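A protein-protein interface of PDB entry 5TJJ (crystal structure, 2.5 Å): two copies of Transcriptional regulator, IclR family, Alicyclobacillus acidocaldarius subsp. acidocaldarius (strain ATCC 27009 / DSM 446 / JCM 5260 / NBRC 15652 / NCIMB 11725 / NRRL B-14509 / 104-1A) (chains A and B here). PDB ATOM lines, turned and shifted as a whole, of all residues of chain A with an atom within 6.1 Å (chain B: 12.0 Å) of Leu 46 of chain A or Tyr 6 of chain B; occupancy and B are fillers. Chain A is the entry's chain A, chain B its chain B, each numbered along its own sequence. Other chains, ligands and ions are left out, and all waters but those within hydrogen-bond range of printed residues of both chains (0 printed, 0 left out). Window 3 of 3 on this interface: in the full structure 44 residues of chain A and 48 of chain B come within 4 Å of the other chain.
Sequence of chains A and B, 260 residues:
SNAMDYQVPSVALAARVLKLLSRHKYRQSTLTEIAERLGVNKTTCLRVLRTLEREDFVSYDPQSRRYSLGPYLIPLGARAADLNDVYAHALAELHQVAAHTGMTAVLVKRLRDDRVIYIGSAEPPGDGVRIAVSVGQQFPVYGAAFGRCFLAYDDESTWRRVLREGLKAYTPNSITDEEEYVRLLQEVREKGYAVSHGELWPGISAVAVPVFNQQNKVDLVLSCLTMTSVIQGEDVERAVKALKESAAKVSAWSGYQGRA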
ATOM      1  N   LEU A  31      22.061  -1.537  -9.125  1.00  0.00           N
ATOM      2  CA  LEU A  31      22.452  -2.414 -10.207  1.00  0.00           C
ATOM      3  C   LEU A  31      23.140  -3.646  -9.614  1.00  0.00           C
ATOM      4  O   LEU A  31      22.823  -4.766 -10.011  1.00  0.00           O
ATOM      5  CB  LEU A  31      23.335  -1.674 -11.219  1.00  0.00           C
ATOM      6  CG  LEU A  31      24.003  -2.465 -12.345  1.00  0.00           C
ATOM      7  CD1 LEU A  31      22.939  -3.123 -13.194  1.00  0.00           C
ATOM      8  CD2 LEU A  31      24.909  -1.584 -13.190  1.00  0.00           C
ATOM      9  N   ASN A  41      25.639 -11.375 -15.055  1.00  0.00           N
ATOM     10  CA  ASN A  41      26.677 -10.380 -15.254  1.00  0.00           C
ATOM     11  C   ASN A  41      26.084  -8.948 -15.227  1.00  0.00           C
ATOM     12  O   ASN A  41      25.093  -8.680 -15.911  1.00  0.00           O
ATOM     13  CB  ASN A  41      27.363 -10.705 -16.582  1.00  0.00           C
ATOM     14  CG  ASN A  41      28.103  -9.544 -17.155  1.00  0.00           C
ATOM     15  OD1 ASN A  41      27.502  -8.660 -17.765  1.00  0.00           O
ATOM     16  ND2 ASN A  41      29.413  -9.535 -16.975  1.00  0.00           N
ATOM     17  N   LYS A  42      26.698  -8.051 -14.444  1.00  0.00           N
ATOM     18  CA  LYS A  42      26.190  -6.665 -14.251  1.00  0.00           C
ATOM     19  C   LYS A  42      26.011  -5.853 -15.536  1.00  0.00           C
ATOM     20  O   LYS A  42      25.066  -5.093 -15.644  1.00  0.00           O
ATOM     21  CB  LYS A  42      27.088  -5.858 -13.299  1.00  0.00           C
ATOM     22  CG  LYS A  42      26.803  -6.117 -11.836  1.00  0.00           C
ATOM     23  CD  LYS A  42      27.896  -5.568 -10.922  1.00  0.00           C
ATOM     24  CE  LYS A  42      27.683  -4.089 -10.640  1.00  0.00           C
ATOM     25  NZ  LYS A  42      28.772  -3.502  -9.801  1.00  0.00           N
ATOM     26  N   THR A  43      26.939  -5.983 -16.480  1.00  0.00           N
ATOM     27  CA  THR A  43      26.811  -5.306 -17.762  1.00  0.00           C
ATOM     28  C   THR A  43      25.567  -5.754 -18.518  1.00  0.00           C
ATOM     29  O   THR A  43      24.801  -4.933 -18.970  1.00  0.00           O
ATOM     30  CB  THR A  43      28.066  -5.526 -18.624  1.00  0.00           C
ATOM     31  OG1 THR A  43      29.177  -4.942 -17.950  1.00  0.00           O
ATOM     32  CG2 THR A  43      27.923  -4.885 -20.016  1.00  0.00           C
ATOM     33  N   THR A  44      25.367  -7.060 -18.636  1.00  0.00           N
ATOM     34  CA  THR A  44      24.147  -7.628 -19.232  1.00  0.00           C
ATOM     35  C   THR A  44      22.903  -6.989 -18.630  1.00  0.00           C
ATOM     36  O   THR A  44      22.018  -6.546 -19.360  1.00  0.00           O
ATOM     37  CB  THR A  44      24.125  -9.170 -19.062  1.00  0.00           C
ATOM     38  OG1 THR A  44      25.360  -9.706 -19.541  1.00  0.00           O
ATOM     39  CG2 THR A  44      23.008  -9.803 -19.836  1.00  0.00           C
ATOM     40  N   CYS A  45      22.866  -6.906 -17.301  1.00  0.00           N
ATOM     41  CA  CYS A  45      21.781  -6.226 -16.578  1.00  0.00           C
ATOM     42  C   CYS A  45      21.580  -4.762 -16.893  1.00  0.00           C
ATOM     43  O   CYS A  45      20.449  -4.292 -16.920  1.00  0.00           O
ATOM     44  CB  CYS A  45      22.033  -6.262 -15.079  1.00  0.00           C
ATOM     45  SG  CYS A  45      21.404  -7.734 -14.319  1.00  0.00           S
ATOM     46  N   LEU A  46      22.676  -4.033 -17.038  1.00  0.00           N
ATOM     47  CA  LEU A  46      22.584  -2.604 -17.273  1.00  0.00           C
ATOM     48  C   LEU A  46      21.849  -2.352 -18.583  1.00  0.00           C
ATOM     49  O   LEU A  46      20.899  -1.577 -18.616  1.00  0.00           O
ATOM     50  CB  LEU A  46      23.970  -1.913 -17.265  1.00  0.00           C
ATOM     51  CG  LEU A  46      23.922  -0.376 -17.198  1.00  0.00           C
ATOM     52  CD1 LEU A  46      23.002   0.116 -16.062  1.00  0.00           C
ATOM     53  CD2 LEU A  46      25.299   0.266 -17.092  1.00  0.00           C
ATOM     54  N   ARG A  47      22.267  -3.050 -19.633  1.00  0.00           N
ATOM     55  CA  ARG A  47      21.684  -2.842 -20.948  1.00  0.00           C
ATOM     56  C   ARG A  47      20.155  -3.063 -20.969  1.00  0.00           C
ATOM     57  O   ARG A  47      19.412  -2.289 -21.590  1.00  0.00           O
ATOM     58  CB  ARG A  47      22.321  -3.770 -21.976  1.00  0.00           C
ATOM     59  CG  ARG A  47      23.779  -3.539 -22.296  1.00  0.00           C
ATOM     60  CD  ARG A  47      24.172  -4.430 -23.472  1.00  0.00           C
ATOM     61  NE  ARG A  47      25.567  -4.914 -23.398  1.00  0.00           N
ATOM     62  CZ  ARG A  47      25.963  -6.162 -23.082  1.00  0.00           C
ATOM     63  NH1 ARG A  47      25.084  -7.129 -22.762  1.00  0.00           N
ATOM     64  NH2 ARG A  47      27.266  -6.437 -23.081  1.00  0.00           N
ATOM     65  N   VAL A  48      19.708  -4.108 -20.285  1.00  0.00           N
ATOM     66  CA  VAL A  48      18.293  -4.439 -20.200  1.00  0.00           C
ATOM     67  C   VAL A  48      17.532  -3.401 -19.390  1.00  0.00           C
ATOM     68  O   VAL A  48      16.510  -2.869 -19.842  1.00  0.00           O
ATOM     69  CB  VAL A  48      18.134  -5.840 -19.581  1.00  0.00           C
ATOM     70  CG1 VAL A  48      16.703  -6.120 -19.131  1.00  0.00           C
ATOM     71  CG2 VAL A  48      18.633  -6.890 -20.576  1.00  0.00           C
ATOM     72  N   LEU A  49      18.049  -3.115 -18.192  1.00  0.00           N
ATOM     73  CA  LEU A  49      17.514  -2.049 -17.333  1.00  0.00           C
ATOM     74  C   LEU A  49      17.369  -0.711 -18.039  1.00  0.00           C
ATOM     75  O   LEU A  49      16.315  -0.098 -17.988  1.00  0.00           O
ATOM     76  CB  LEU A  49      18.389  -1.860 -16.091  1.00  0.00           C
ATOM     77  CG  LEU A  49      18.188  -2.909 -14.987  1.00  0.00           C
ATOM     78  CD1 LEU A  49      19.344  -2.894 -14.001  1.00  0.00           C
ATOM     79  CD2 LEU A  49      16.885  -2.666 -14.260  1.00  0.00           C
ATOM     80  N   ARG A  50      18.426  -0.249 -18.685  1.00  0.00           N
ATOM     81  CA  ARG A  50      18.358   1.026 -19.384  1.00  0.00           C
ATOM     82  C   ARG A  50      17.362   0.966 -20.577  1.00  0.00           C
ATOM     83  O   ARG A  50      16.710   1.951 -20.892  1.00  0.00           O
ATOM     84  CB  ARG A  50      19.761   1.495 -19.819  1.00  0.00           C
ATOM     85  CG  ARG A  50      20.551   2.212 -18.711  1.00  0.00           C
ATOM     86  CD  ARG A  50      22.004   2.486 -19.136  1.00  0.00           C
ATOM     87  NE  ARG A  50      22.652   3.697 -18.572  1.00  0.00           N
ATOM     88  CZ  ARG A  50      23.047   4.791 -19.253  1.00  0.00           C
ATOM     89  NH1 ARG A  50      22.850   4.902 -20.570  1.00  0.00           N
ATOM     90  NH2 ARG A  50      23.637   5.800 -18.606  1.00  0.00           N
ATOM     91  N   THR A  51      17.236  -0.193 -21.219  1.00  0.00           N
ATOM     92  CA  THR A  51      16.274  -0.368 -22.312  1.00  0.00           C
ATOM     93  C   THR A  51      14.849  -0.290 -21.763  1.00  0.00           C
ATOM     94  O   THR A  51      14.010   0.423 -22.329  1.00  0.00           O
ATOM     95  CB  THR A  51      16.511  -1.696 -23.050  1.00  0.00           C
ATOM     96  OG1 THR A  51      17.868  -1.738 -23.472  1.00  0.00           O
ATOM     97  CG2 THR A  51      15.630  -1.830 -24.263  1.00  0.00           C
ATOM     98  N   TYR A  67      16.814   1.343  -8.983  1.00  0.00           N
ATOM     99  CA  TYR A  67      15.815   1.086 -10.000  1.00  0.00           C
ATOM    100  C   TYR A  67      14.546   0.554  -9.341  1.00  0.00           C
ATOM    101  O   TYR A  67      14.587  -0.086  -8.278  1.00  0.00           O
ATOM    102  CB  TYR A  67      16.326   0.045 -11.020  1.00  0.00           C
ATOM    103  CG  TYR A  67      17.549   0.472 -11.821  1.00  0.00           C
ATOM    104  CD1 TYR A  67      17.417   1.123 -13.051  1.00  0.00           C
ATOM    105  CD2 TYR A  67      18.841   0.228 -11.353  1.00  0.00           C
ATOM    106  CE1 TYR A  67      18.540   1.505 -13.793  1.00  0.00           C
ATOM    107  CE2 TYR A  67      19.959   0.623 -12.080  1.00  0.00           C
ATOM    108  CZ  TYR A  67      19.809   1.257 -13.305  1.00  0.00           C
ATOM    109  OH  TYR A  67      20.928   1.655 -14.022  1.00  0.00           O
ATOM    110  N   TYR B   6      22.875   2.668 -25.053  1.00  0.00           N
ATOM    111  CA  TYR B   6      22.464   1.363 -25.667  1.00  0.00           C
ATOM    112  C   TYR B   6      20.976   1.023 -25.545  1.00  0.00           C
ATOM    113  O   TYR B   6      20.241   1.552 -24.709  1.00  0.00           O
ATOM    114  CB  TYR B   6      23.302   0.144 -25.180  1.00  0.00           C
ATOM    115  CG  TYR B   6      24.013   0.254 -23.835  1.00  0.00           C
ATOM    116  CD1 TYR B   6      25.401   0.083 -23.753  1.00  0.00           C
ATOM    117  CD2 TYR B   6      23.311   0.490 -22.648  1.00  0.00           C
ATOM    118  CE1 TYR B   6      26.084   0.163 -22.547  1.00  0.00           C
ATOM    119  CE2 TYR B   6      23.987   0.576 -21.428  1.00  0.00           C
ATOM    120  CZ  TYR B   6      25.377   0.412 -21.384  1.00  0.00           C
ATOM    121  OH  TYR B   6      26.095   0.487 -20.208  1.00  0.00           O
ATOM    122  N   GLN B   7      20.578   0.116 -26.430  1.00  0.00           N
ATOM    123  CA  GLN B   7      19.235  -0.422 -26.488  1.00  0.00           C
ATOM    124  C   GLN B   7      19.367  -1.885 -26.908  1.00  0.00           C
ATOM    125  O   GLN B   7      20.114  -2.199 -27.838  1.00  0.00           O
ATOM    126  CB  GLN B   7      18.414   0.355 -27.504  1.00  0.00           C
ATOM    127  CG  GLN B   7      16.935   0.058 -27.446  1.00  0.00           C
ATOM    128  CD  GLN B   7      16.113   1.046 -28.249  1.00  0.00           C
ATOM    129  OE1 GLN B   7      15.112   1.577 -27.772  1.00  0.00           O
ATOM    130  NE2 GLN B   7      16.541   1.297 -29.476  1.00  0.00           N
ATOM    131  N   VAL B   8      18.692  -2.776 -26.186  1.00  0.00           N
ATOM    132  CA  VAL B   8      18.635  -4.198 -26.547  1.00  0.00           C
ATOM    133  C   VAL B   8      17.438  -4.392 -27.477  1.00  0.00           C
ATOM    134  O   VAL B   8      16.301  -4.327 -27.019  1.00  0.00           O
ATOM    135  CB  VAL B   8      18.514  -5.091 -25.299  1.00  0.00           C
ATOM    136  CG1 VAL B   8      18.472  -6.570 -25.690  1.00  0.00           C
ATOM    137  CG2 VAL B   8      19.674  -4.788 -24.342  1.00  0.00           C
ATOM    138  N   PRO B   9      17.691  -4.610 -28.787  1.00  0.00           N
ATOM    139  CA  PRO B   9      16.597  -4.625 -29.764  1.00  0.00           C
ATOM    140  C   PRO B   9      15.394  -5.504 -29.430  1.00  0.00           C
ATOM    141  O   PRO B   9      14.264  -5.086 -29.682  1.00  0.00           O
ATOM    142  CB  PRO B   9      17.284  -5.107 -31.049  1.00  0.00           C
ATOM    143  CG  PRO B   9      18.681  -4.618 -30.900  1.00  0.00           C
ATOM    144  CD  PRO B   9      19.005  -4.771 -29.450  1.00  0.00           C
ATOM    145  N   SER B  10      15.632  -6.690 -28.870  1.00  0.00           N
ATOM    146  CA  SER B  10      14.535  -7.616 -28.497  1.00  0.00           C
ATOM    147  C   SER B  10      13.651  -7.131 -27.358  1.00  0.00           C
ATOM    148  O   SER B  10      12.432  -7.308 -27.404  1.00  0.00           O
ATOM    149  CB  SER B  10      15.092  -8.972 -28.115  1.00  0.00           C
ATOM    150  OG  SER B  10      15.766  -9.529 -29.226  1.00  0.00           O
ATOM    151  N   VAL B  11      14.278  -6.537 -26.338  1.00  0.00           N
ATOM    152  CA  VAL B  11      13.564  -5.985 -25.162  1.00  0.00           C
ATOM    153  C   VAL B  11      12.723  -4.804 -25.611  1.00  0.00           C
ATOM    154  O   VAL B  11      11.552  -4.717 -25.226  1.00  0.00           O
ATOM    155  CB  VAL B  11      14.522  -5.558 -24.018  1.00  0.00           C
ATOM    156  CG1 VAL B  11      13.759  -4.915 -22.859  1.00  0.00           C
ATOM    157  CG2 VAL B  11      15.342  -6.749 -23.536  1.00  0.00           C
ATOM    158  N   ALA B  12      13.312  -3.918 -26.432  1.00  0.00           N
ATOM    159  CA  ALA B  12      12.560  -2.817 -27.044  1.00  0.00           C
ATOM    160  C   ALA B  12      11.384  -3.361 -27.879  1.00  0.00           C
ATOM    161  O   ALA B  12      10.281  -2.827 -27.804  1.00  0.00           O
ATOM    162  CB  ALA B  12      13.468  -1.959 -27.902  1.00  0.00           C
ATOM    163  N   LEU B  13      11.606  -4.444 -28.635  1.00  0.00           N
ATOM    164  CA  LEU B  13      10.523  -5.071 -29.381  1.00  0.00           C
ATOM    165  C   LEU B  13       9.447  -5.667 -28.450  1.00  0.00           C
ATOM    166  O   LEU B  13       8.254  -5.524 -28.715  1.00  0.00           O
ATOM    167  CB  LEU B  13      11.052  -6.128 -30.359  1.00  0.00           C
ATOM    168  CG  LEU B  13       9.974  -6.702 -31.293  1.00  0.00           C
ATOM    169  CD1 LEU B  13       9.273  -5.557 -32.035  1.00  0.00           C
ATOM    170  CD2 LEU B  13      10.553  -7.727 -32.270  1.00  0.00           C
ATOM    171  N   ARG B 112       8.698   9.836 -22.117  1.00  0.00           N
ATOM    172  CA  ARG B 112       9.674  10.291 -23.085  1.00  0.00           C
ATOM    173  C   ARG B 112       9.043  10.563 -24.455  1.00  0.00           C
ATOM    174  O   ARG B 112       7.940  10.119 -24.722  1.00  0.00           O
ATOM    175  CB  ARG B 112      10.784   9.274 -23.182  1.00  0.00           C
ATOM    176  CG  ARG B 112      11.650   9.278 -21.932  1.00  0.00           C
ATOM    177  CD  ARG B 112      12.101   7.880 -21.579  1.00  0.00           C
ATOM    178  NE  ARG B 112      13.117   7.905 -20.538  1.00  0.00           N
ATOM    179  CZ  ARG B 112      14.401   8.210 -20.727  1.00  0.00           C
ATOM    180  NH1 ARG B 112      14.863   8.539 -21.940  1.00  0.00           N
ATOM    181  NH2 ARG B 112      15.225   8.187 -19.688  1.00  0.00           N
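OG1 of Thr 51 of chain A sits at hydrogen-bond distance from N of Val 8 of chain B (3.0 Å).
O of Arg 47 of chain A is in hydrogen-bond range of OG1 of Thr 51 of chain A (2.5 Å).
Among the printed residues, pairs that only touch across the chains: Leu 46 of chain A with Tyr 6 of chain B (3.2 Å), Thr 51 of chain A with Gln 7 of chain B (3.6 Å), Arg 50 of chain A with Tyr 6 of chain B (3.6 Å), Arg 47 of chain A with Val 8 of chain B (3.7 Å), Thr 51 of chain A with Ala 12 of chain B (3.8 Å) and Thr 51 of chain A with Val 11 of chain B (3.9 Å).
Of chain B, only Tyr 6 comes within 4 Å of Leu 46 of chain A.
Of chain A, only Leu 46 (3.2 Å) and Arg 50 (3.6 Å) come within 4 Å of Tyr 6 of chain B.
No residue of chain B comes within 4 Å of Leu 31 of chain A.
No residue of chain B comes within 4 Å of Thr 43 of chain A.
No residue of chain B comes within 4 Å of Thr 44 of chain A.
Arg 47 of chain A touches just one residue of chain B: Val 8 (3.7 Å).
No residue of chain B comes within 4 Å of Val 48 of chain A.
No residue of chain B comes within 4 Å of Leu 49 of chain A.
Arg 50 of chain A touches one residue of chain B.
Of chain B, only Gln 7, Val 8, Val 11 and Ala 12 come within 4 Å of Thr 51 of chain A.
Printed residues of chain A within 4 Å of Val 8 of chain B: Arg 47 and Thr 51.
Printed residues of chain A within 4 Å of Val 11 of chain B: Thr 51.
Pro 9 of chain B touches none of the printed residues of chain A.
The nearest residue of chain A that does not touch Tyr 6 of chain B is Arg 47 of chain A (4.1 Å).
Of the 13 printed residues of chain A, 4 touch a printed residue of chain B.
Printed residues of chain A that touch a printed residue of chain B: Leu 46, Arg 47, Arg 50 and Thr 51.
Hydrophobic or aromatic side chains of chain B within 4 Å of the printed part of chain A: Tyr 6, Val 8 and Val 11.
Among the printed residues, no Asp or Glu carboxylate lies within 4 Å of a Lys or Arg side-chain nitrogen of the other chain.
No position is printed for both chains.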
